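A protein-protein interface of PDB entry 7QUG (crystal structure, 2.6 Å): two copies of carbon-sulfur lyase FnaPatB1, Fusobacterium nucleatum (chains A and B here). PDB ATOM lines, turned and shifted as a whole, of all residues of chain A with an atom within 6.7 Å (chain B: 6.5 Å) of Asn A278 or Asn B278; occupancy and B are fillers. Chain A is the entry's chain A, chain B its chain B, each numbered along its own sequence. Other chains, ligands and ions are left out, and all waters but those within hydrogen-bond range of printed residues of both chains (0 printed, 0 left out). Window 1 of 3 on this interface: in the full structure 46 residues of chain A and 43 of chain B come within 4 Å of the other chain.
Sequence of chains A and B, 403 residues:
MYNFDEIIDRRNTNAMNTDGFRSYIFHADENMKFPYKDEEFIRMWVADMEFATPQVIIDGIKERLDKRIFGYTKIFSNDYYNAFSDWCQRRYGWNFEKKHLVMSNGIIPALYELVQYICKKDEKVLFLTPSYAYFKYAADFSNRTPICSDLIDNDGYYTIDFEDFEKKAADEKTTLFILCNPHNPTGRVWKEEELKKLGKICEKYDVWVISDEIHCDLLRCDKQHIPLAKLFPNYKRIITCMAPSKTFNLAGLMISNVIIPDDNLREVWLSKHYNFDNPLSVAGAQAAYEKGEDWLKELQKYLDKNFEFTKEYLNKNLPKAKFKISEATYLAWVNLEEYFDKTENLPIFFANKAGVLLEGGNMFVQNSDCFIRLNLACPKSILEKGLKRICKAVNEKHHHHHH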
ATOM      1  N   THR A  73       2.203  21.052  36.015  1.00  0.00           N
ATOM      2  CA  THR A  73       0.808  21.064  36.429  1.00  0.00           C
ATOM      3  C   THR A  73       0.509  19.878  37.334  1.00  0.00           C
ATOM      4  O   THR A  73       0.808  18.731  36.981  1.00  0.00           O
ATOM      5  CB  THR A  73      -0.113  21.023  35.207  1.00  0.00           C
ATOM      6  OG1 THR A  73       0.092  22.202  34.430  1.00  0.00           O
ATOM      7  CG2 THR A  73      -1.583  20.913  35.626  1.00  0.00           C
ATOM      8  N   ALA A 251      -9.975   8.780  24.902  1.00  0.00           N
ATOM      9  CA  ALA A 251      -8.818   7.889  25.128  1.00  0.00           C
ATOM     10  C   ALA A 251      -7.486   8.605  24.888  1.00  0.00           C
ATOM     11  O   ALA A 251      -6.534   8.439  25.658  1.00  0.00           O
ATOM     12  CB  ALA A 251      -8.890   6.636  24.232  1.00  0.00           C
ATOM     13  N   GLY A 252      -7.404   9.413  23.830  1.00  0.00           N
ATOM     14  CA  GLY A 252      -6.178  10.134  23.561  1.00  0.00           C
ATOM     15  C   GLY A 252      -5.712  11.014  24.708  1.00  0.00           C
ATOM     16  O   GLY A 252      -4.520  11.309  24.812  1.00  0.00           O
ATOM     17  N   LEU A 253      -6.637  11.486  25.564  1.00  0.00           N
ATOM     18  CA  LEU A 253      -6.213  12.394  26.627  1.00  0.00           C
ATOM     19  C   LEU A 253      -5.466  11.687  27.739  1.00  0.00           C
ATOM     20  O   LEU A 253      -4.863  12.372  28.573  1.00  0.00           O
ATOM     21  CB  LEU A 253      -7.407  13.136  27.219  1.00  0.00           C
ATOM     22  CG  LEU A 253      -8.177  14.076  26.286  1.00  0.00           C
ATOM     23  CD1 LEU A 253      -9.243  14.812  27.067  1.00  0.00           C
ATOM     24  CD2 LEU A 253      -7.238  15.060  25.599  1.00  0.00           C
ATOM     25  N   MET A 254      -5.482  10.348  27.758  1.00  0.00           N
ATOM     26  CA  MET A 254      -4.707   9.540  28.696  1.00  0.00           C
ATOM     27  C   MET A 254      -4.840  10.068  30.126  1.00  0.00           C
ATOM     28  O   MET A 254      -3.872  10.479  30.765  1.00  0.00           O
ATOM     29  CB  MET A 254      -3.238   9.476  28.279  1.00  0.00           C
ATOM     30  CG  MET A 254      -3.066   9.150  26.817  1.00  0.00           C
ATOM     31  SD  MET A 254      -1.383   8.703  26.285  1.00  0.00           S
ATOM     32  CE  MET A 254      -0.357  10.038  26.857  1.00  0.00           C
ATOM     33  N   ILE A 255      -6.064  10.035  30.635  1.00  0.00           N
ATOM     34  CA  ILE A 255      -6.319  10.494  31.996  1.00  0.00           C
ATOM     35  C   ILE A 255      -7.456   9.658  32.569  1.00  0.00           C
ATOM     36  O   ILE A 255      -8.482   9.439  31.916  1.00  0.00           O
ATOM     37  CB  ILE A 255      -6.613  12.009  32.052  1.00  0.00           C
ATOM     38  CG1 ILE A 255      -6.727  12.493  33.497  1.00  0.00           C
ATOM     39  CG2 ILE A 255      -7.843  12.384  31.241  1.00  0.00           C
ATOM     40  CD1 ILE A 255      -6.642  14.014  33.602  1.00  0.00           C
ATOM     41  N   PHE A 276       2.742  14.444  37.879  1.00  0.00           N
ATOM     42  CA  PHE A 276       2.342  15.641  37.154  1.00  0.00           C
ATOM     43  C   PHE A 276       1.232  15.283  36.182  1.00  0.00           C
ATOM     44  O   PHE A 276       1.177  14.164  35.671  1.00  0.00           O
ATOM     45  CB  PHE A 276       3.519  16.262  36.389  1.00  0.00           C
ATOM     46  CG  PHE A 276       4.492  16.991  37.268  1.00  0.00           C
ATOM     47  CD1 PHE A 276       4.040  17.900  38.225  1.00  0.00           C
ATOM     48  CD2 PHE A 276       5.859  16.777  37.144  1.00  0.00           C
ATOM     49  CE1 PHE A 276       4.937  18.572  39.049  1.00  0.00           C
ATOM     50  CE2 PHE A 276       6.766  17.451  37.963  1.00  0.00           C
ATOM     51  CZ  PHE A 276       6.303  18.351  38.917  1.00  0.00           C
ATOM     52  N   ASP A 277       0.367  16.252  35.904  1.00  0.00           N
ATOM     53  CA  ASP A 277      -0.793  16.037  35.054  1.00  0.00           C
ATOM     54  C   ASP A 277      -0.703  16.918  33.822  1.00  0.00           C
ATOM     55  O   ASP A 277      -0.071  17.974  33.854  1.00  0.00           O
ATOM     56  CB  ASP A 277      -2.089  16.359  35.794  1.00  0.00           C
ATOM     57  CG  ASP A 277      -2.265  15.531  37.023  1.00  0.00           C
ATOM     58  OD1 ASP A 277      -2.335  14.292  36.872  1.00  0.00           O
ATOM     59  OD2 ASP A 277      -2.354  16.126  38.121  1.00  0.00           O
ATOM     60  N   ASN A 278      -1.343  16.479  32.738  1.00  0.00           N
ATOM     61  CA  ASN A 278      -1.450  17.306  31.535  1.00  0.00           C
ATOM     62  C   ASN A 278      -2.585  18.307  31.709  1.00  0.00           C
ATOM     63  O   ASN A 278      -3.738  17.894  31.883  1.00  0.00           O
ATOM     64  CB  ASN A 278      -1.698  16.445  30.298  1.00  0.00           C
ATOM     65  CG  ASN A 278      -1.739  17.258  28.997  1.00  0.00           C
ATOM     66  OD1 ASN A 278      -2.248  18.372  28.959  1.00  0.00           O
ATOM     67  ND2 ASN A 278      -1.197  16.691  27.929  1.00  0.00           N
ATOM     68  N   PRO A 279      -2.317  19.615  31.672  1.00  0.00           N
ATOM     69  CA  PRO A 279      -3.411  20.578  31.907  1.00  0.00           C
ATOM     70  C   PRO A 279      -4.539  20.488  30.886  1.00  0.00           C
ATOM     71  O   PRO A 279      -5.716  20.639  31.251  1.00  0.00           O
ATOM     72  CB  PRO A 279      -2.700  21.941  31.870  1.00  0.00           C
ATOM     73  CG  PRO A 279      -1.397  21.684  31.144  1.00  0.00           C
ATOM     74  CD  PRO A 279      -1.016  20.271  31.447  1.00  0.00           C
ATOM     75  N   LEU A 280      -4.232  20.215  29.619  1.00  0.00           N
ATOM     76  CA  LEU A 280      -5.305  20.097  28.647  1.00  0.00           C
ATOM     77  C   LEU A 280      -6.163  18.870  28.947  1.00  0.00           C
ATOM     78  O   LEU A 280      -7.389  18.898  28.785  1.00  0.00           O
ATOM     79  CB  LEU A 280      -4.723  20.047  27.234  1.00  0.00           C
ATOM     80  CG  LEU A 280      -3.777  21.197  26.885  1.00  0.00           C
ATOM     81  CD1 LEU A 280      -3.274  21.115  25.454  1.00  0.00           C
ATOM     82  CD2 LEU A 280      -4.481  22.513  27.114  1.00  0.00           C
ATOM     83  N   SER A 281      -5.537  17.802  29.430  1.00  0.00           N
ATOM     84  CA  SER A 281      -6.269  16.583  29.745  1.00  0.00           C
ATOM     85  C   SER A 281      -7.156  16.771  30.978  1.00  0.00           C
ATOM     86  O   SER A 281      -8.297  16.294  31.009  1.00  0.00           O
ATOM     87  CB  SER A 281      -5.272  15.435  29.944  1.00  0.00           C
ATOM     88  OG  SER A 281      -4.539  15.183  28.746  1.00  0.00           O
ATOM     89  N   VAL A 282      -6.641  17.450  32.011  1.00  0.00           N
ATOM     90  CA  VAL A 282      -7.457  17.737  33.183  1.00  0.00           C
ATOM     91  C   VAL A 282      -8.620  18.639  32.801  1.00  0.00           C
ATOM     92  O   VAL A 282      -9.757  18.441  33.251  1.00  0.00           O
ATOM     93  CB  VAL A 282      -6.602  18.368  34.287  1.00  0.00           C
ATOM     94  CG1 VAL A 282      -7.495  18.783  35.450  1.00  0.00           C
ATOM     95  CG2 VAL A 282      -5.516  17.400  34.722  1.00  0.00           C
ATOM     96  N   ALA A 283      -8.354  19.631  31.942  1.00  0.00           N
ATOM     97  CA  ALA A 283      -9.400  20.551  31.515  1.00  0.00           C
ATOM     98  C   ALA A 283     -10.495  19.810  30.769  1.00  0.00           C
ATOM     99  O   ALA A 283     -11.685  20.099  30.950  1.00  0.00           O
ATOM    100  CB  ALA A 283      -8.815  21.655  30.631  1.00  0.00           C
ATOM    101  N   THR B  73      -4.236   6.979  20.022  1.00  0.00           N
ATOM    102  CA  THR B  73      -3.378   7.767  19.159  1.00  0.00           C
ATOM    103  C   THR B  73      -1.955   7.265  19.278  1.00  0.00           C
ATOM    104  O   THR B  73      -1.436   7.100  20.387  1.00  0.00           O
ATOM    105  CB  THR B  73      -3.478   9.269  19.522  1.00  0.00           C
ATOM    106  OG1 THR B  73      -4.794   9.760  19.207  1.00  0.00           O
ATOM    107  CG2 THR B  73      -2.424  10.095  18.804  1.00  0.00           C
ATOM    108  N   GLY B 252       3.855  20.916  30.738  1.00  0.00           N
ATOM    109  CA  GLY B 252       2.573  20.291  30.996  1.00  0.00           C
ATOM    110  C   GLY B 252       2.154  19.292  29.930  1.00  0.00           C
ATOM    111  O   GLY B 252       1.448  18.324  30.237  1.00  0.00           O
ATOM    112  N   LEU B 253       2.592  19.486  28.671  1.00  0.00           N
ATOM    113  CA  LEU B 253       2.143  18.567  27.622  1.00  0.00           C
ATOM    114  C   LEU B 253       2.793  17.184  27.716  1.00  0.00           C
ATOM    115  O   LEU B 253       2.380  16.289  26.976  1.00  0.00           O
ATOM    116  CB  LEU B 253       2.375  19.153  26.216  1.00  0.00           C
ATOM    117  CG  LEU B 253       1.608  20.462  25.947  1.00  0.00           C
ATOM    118  CD1 LEU B 253       1.681  20.963  24.479  1.00  0.00           C
ATOM    119  CD2 LEU B 253       0.174  20.395  26.448  1.00  0.00           C
ATOM    120  N   MET B 254       3.796  17.004  28.577  1.00  0.00           N
ATOM    121  CA  MET B 254       4.423  15.712  28.875  1.00  0.00           C
ATOM    122  C   MET B 254       4.768  14.927  27.603  1.00  0.00           C
ATOM    123  O   MET B 254       4.247  13.841  27.323  1.00  0.00           O
ATOM    124  CB  MET B 254       3.540  14.921  29.833  1.00  0.00           C
ATOM    125  CG  MET B 254       3.139  15.790  31.013  1.00  0.00           C
ATOM    126  SD  MET B 254       2.366  14.963  32.403  1.00  0.00           S
ATOM    127  CE  MET B 254       1.042  14.158  31.511  1.00  0.00           C
ATOM    128  N   ILE B 255       5.678  15.508  26.829  1.00  0.00           N
ATOM    129  CA  ILE B 255       6.120  14.920  25.573  1.00  0.00           C
ATOM    130  C   ILE B 255       7.583  15.293  25.354  1.00  0.00           C
ATOM    131  O   ILE B 255       7.955  16.467  25.407  1.00  0.00           O
ATOM    132  CB  ILE B 255       5.199  15.376  24.414  1.00  0.00           C
ATOM    133  CG1 ILE B 255       5.550  14.691  23.095  1.00  0.00           C
ATOM    134  CG2 ILE B 255       5.171  16.894  24.266  1.00  0.00           C
ATOM    135  CD1 ILE B 255       4.416  14.783  22.074  1.00  0.00           C
ATOM    136  N   PHE B 276       1.137   4.744  23.712  1.00  0.00           N
ATOM    137  CA  PHE B 276       0.122   5.654  23.196  1.00  0.00           C
ATOM    138  C   PHE B 276       0.519   7.094  23.501  1.00  0.00           C
ATOM    139  O   PHE B 276       1.263   7.353  24.450  1.00  0.00           O
ATOM    140  CB  PHE B 276      -1.235   5.328  23.802  1.00  0.00           C
ATOM    141  CG  PHE B 276      -1.852   4.098  23.221  1.00  0.00           C
ATOM    142  CD1 PHE B 276      -1.964   3.953  21.852  1.00  0.00           C
ATOM    143  CD2 PHE B 276      -2.256   3.057  24.034  1.00  0.00           C
ATOM    144  CE1 PHE B 276      -2.515   2.815  21.304  1.00  0.00           C
ATOM    145  CE2 PHE B 276      -2.799   1.914  23.492  1.00  0.00           C
ATOM    146  CZ  PHE B 276      -2.923   1.795  22.120  1.00  0.00           C
ATOM    147  N   ASP B 277       0.074   8.022  22.650  1.00  0.00           N
ATOM    148  CA  ASP B 277       0.406   9.437  22.772  1.00  0.00           C
ATOM    149  C   ASP B 277      -0.837  10.294  22.907  1.00  0.00           C
ATOM    150  O   ASP B 277      -1.909   9.940  22.412  1.00  0.00           O
ATOM    151  CB  ASP B 277       1.177   9.932  21.558  1.00  0.00           C
ATOM    152  CG  ASP B 277       2.460   9.200  21.377  1.00  0.00           C
ATOM    153  OD1 ASP B 277       3.359   9.336  22.244  1.00  0.00           O
ATOM    154  OD2 ASP B 277       2.515   8.422  20.410  1.00  0.00           O
ATOM    155  N   ASN B 278      -0.669  11.451  23.533  1.00  0.00           N
ATOM    156  CA  ASN B 278      -1.748  12.421  23.596  1.00  0.00           C
ATOM    157  C   ASN B 278      -1.782  13.220  22.299  1.00  0.00           C
ATOM    158  O   ASN B 278      -0.831  13.952  22.011  1.00  0.00           O
ATOM    159  CB  ASN B 278      -1.569  13.342  24.796  1.00  0.00           C
ATOM    160  CG  ASN B 278      -2.723  14.337  24.956  1.00  0.00           C
ATOM    161  OD1 ASN B 278      -3.268  14.863  23.967  1.00  0.00           O
ATOM    162  ND2 ASN B 278      -3.097  14.602  26.206  1.00  0.00           N
ATOM    163  N   PRO B 279      -2.855  13.139  21.515  1.00  0.00           N
ATOM    164  CA  PRO B 279      -2.861  13.842  20.225  1.00  0.00           C
ATOM    165  C   PRO B 279      -2.721  15.351  20.380  1.00  0.00           C
ATOM    166  O   PRO B 279      -2.093  15.997  19.527  1.00  0.00           O
ATOM    167  CB  PRO B 279      -4.208  13.437  19.601  1.00  0.00           C
ATOM    168  CG  PRO B 279      -5.055  13.016  20.758  1.00  0.00           C
ATOM    169  CD  PRO B 279      -4.130  12.446  21.792  1.00  0.00           C
ATOM    170  N   LEU B 280      -3.277  15.938  21.446  1.00  0.00           N
ATOM    171  CA  LEU B 280      -3.082  17.368  21.656  1.00  0.00           C
ATOM    172  C   LEU B 280      -1.616  17.661  21.962  1.00  0.00           C
ATOM    173  O   LEU B 280      -1.086  18.690  21.528  1.00  0.00           O
ATOM    174  CB  LEU B 280      -3.995  17.887  22.780  1.00  0.00           C
ATOM    175  CG  LEU B 280      -5.511  17.590  22.713  1.00  0.00           C
ATOM    176  CD1 LEU B 280      -6.265  18.234  23.864  1.00  0.00           C
ATOM    177  CD2 LEU B 280      -6.115  18.015  21.388  1.00  0.00           C
ATOM    178  N   SER B 281      -0.937  16.748  22.664  1.00  0.00           N
ATOM    179  CA  SER B 281       0.478  16.945  22.954  1.00  0.00           C
ATOM    180  C   SER B 281       1.321  16.819  21.693  1.00  0.00           C
ATOM    181  O   SER B 281       2.265  17.595  21.490  1.00  0.00           O
ATOM    182  CB  SER B 281       0.949  15.940  24.002  1.00  0.00           C
ATOM    183  OG  SER B 281       0.331  16.155  25.258  1.00  0.00           O
ATOM    184  N   VAL B 282       1.012  15.833  20.848  1.00  0.00           N
ATOM    185  CA  VAL B 282       1.756  15.670  19.605  1.00  0.00           C
ATOM    186  C   VAL B 282       1.537  16.868  18.698  1.00  0.00           C
ATOM    187  O   VAL B 282       2.474  17.354  18.050  1.00  0.00           O
ATOM    188  CB  VAL B 282       1.369  14.344  18.912  1.00  0.00           C
ATOM    189  CG1 VAL B 282       2.062  14.221  17.561  1.00  0.00           C
ATOM    190  CG2 VAL B 282       1.759  13.182  19.784  1.00  0.00           C
ATOM    191  N   ALA B 283       0.302  17.365  18.640  1.00  0.00           N
ATOM    192  CA  ALA B 283       0.017  18.511  17.781  1.00  0.00           C
ATOM    193  C   ALA B 283       0.804  19.731  18.229  1.00  0.00           C
ATOM    194  O   ALA B 283       1.300  20.498  17.391  1.00  0.00           O
ATOM    195  CB  ALA B 283      -1.481  18.824  17.763  1.00  0.00           C
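Of the 14 printed residues of chain A, 9 touch a printed residue of chain B.
Printed residues of chain A that touch a printed residue of chain B: Gly A252, Leu A253, Met A254, Phe A276, Asp A277, Asn A278, Pro A279, Leu A280 and Ser A281.
Hydrophobic or aromatic side chains of chain B that line the printed part of chain A: Leu B253, Met B254, Pro B279 and Leu B280.
Among the printed residues, no Asp or Glu carboxylate lies within 4 Å of a Lys or Arg side-chain nitrogen of the other chain.
OG of Ser A281 sits at hydrogen-bond distance from O of Leu A253, at 2.8 Å.
The backbone NH (N) of Leu A280 is in hydrogen-bond range of the side-chain amide oxygen (OD1) of Asn A278, 2.8 Å away.
OD1 of Asn A278 lies within hydrogen-bond range of N of Ser A281 (3.4 Å).
N of Asp B277 lies within hydrogen-bond range of O of Thr B73, 2.9 Å away.
The side-chain amide oxygen (OD1) of Asn B278 is in hydrogen-bond range of the backbone NH (N) of Leu B280.
OD1 of Asn B278 is in hydrogen-bond range of N of Ser B281.
Gly A252 touches Asn B278, and with the chains exchanged Asn A278 touches Gly B252.
Gly A252 touches Pro B279, and with the chains exchanged Pro A279 touches Gly B252.
Met A254 touches Asp B277, and with the chains exchanged Asp A277 touches Met B254.
Met A254 touches Asn B278, and with the chains exchanged Asn A278 touches Met B254.
13 positions are printed for both chains.
Of chain B, only Gly B252 (3.3 Å), Leu B253 (3.7 Å), Met B254 (3.5 Å), Asn B278 (3.3 Å) and Ser B281 (3.1 Å) come within 4 Å of Asn A278.
Asn B278 touches just these residues of chain A: Gly A252, Leu A253, Met A254, Asn A278 and Ser A281.
Printed residues of chain A within 4 Å of Ser B281: Asn A278.
Of the printed residues of chain B, Leu A280 touches Leu B253.
Thr A73 touches none of the printed residues of chain B.
Val B282 touches none of the printed residues of chain A.
The nearest residue of chain A that does not touch Asn B278 is Leu A280 (5.8 Å).
The nearest printed residue of chain A that does not touch Leu B253 is Pro A279 (4.6 Å).
Among the printed residues, merely in contact across the chains: Gly A252 with Asn B278, Gly A252 with Pro B279, Asn A278 with Gly B252, Pro A279 with Gly B252, Asn A278 with Met B254, Met A254 with Asn B278, Leu A280 with Leu B253, Leu A253 with Asn B278, Asn A278 with Leu B253, Leu A253 with Leu B280, Met A254 with Asp B277, Gly A252 with Asp B277, Asp A277 with Met B254 and Asp A277 with Gly B252.
ND2 of Asn A278 sits close to ND2 of Asn B278 (3.3 Å).
The side-chain amide nitrogen (ND2) of Asn A278 sits at hydrogen-bond distance from the side-chain hydroxyl (OG) of Ser B281, at 3.1 Å.
The side-chain hydroxyl of Ser A281 sits at hydrogen-bond distance from the side-chain amide nitrogen of Asn B278 (3.0 Å).
The backbone carbonyl oxygen of Phe B276 lies close to the side-chain sulfur of Met A254 (3.5 Å).
SD of Met B254 sits close to O of Phe A276.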
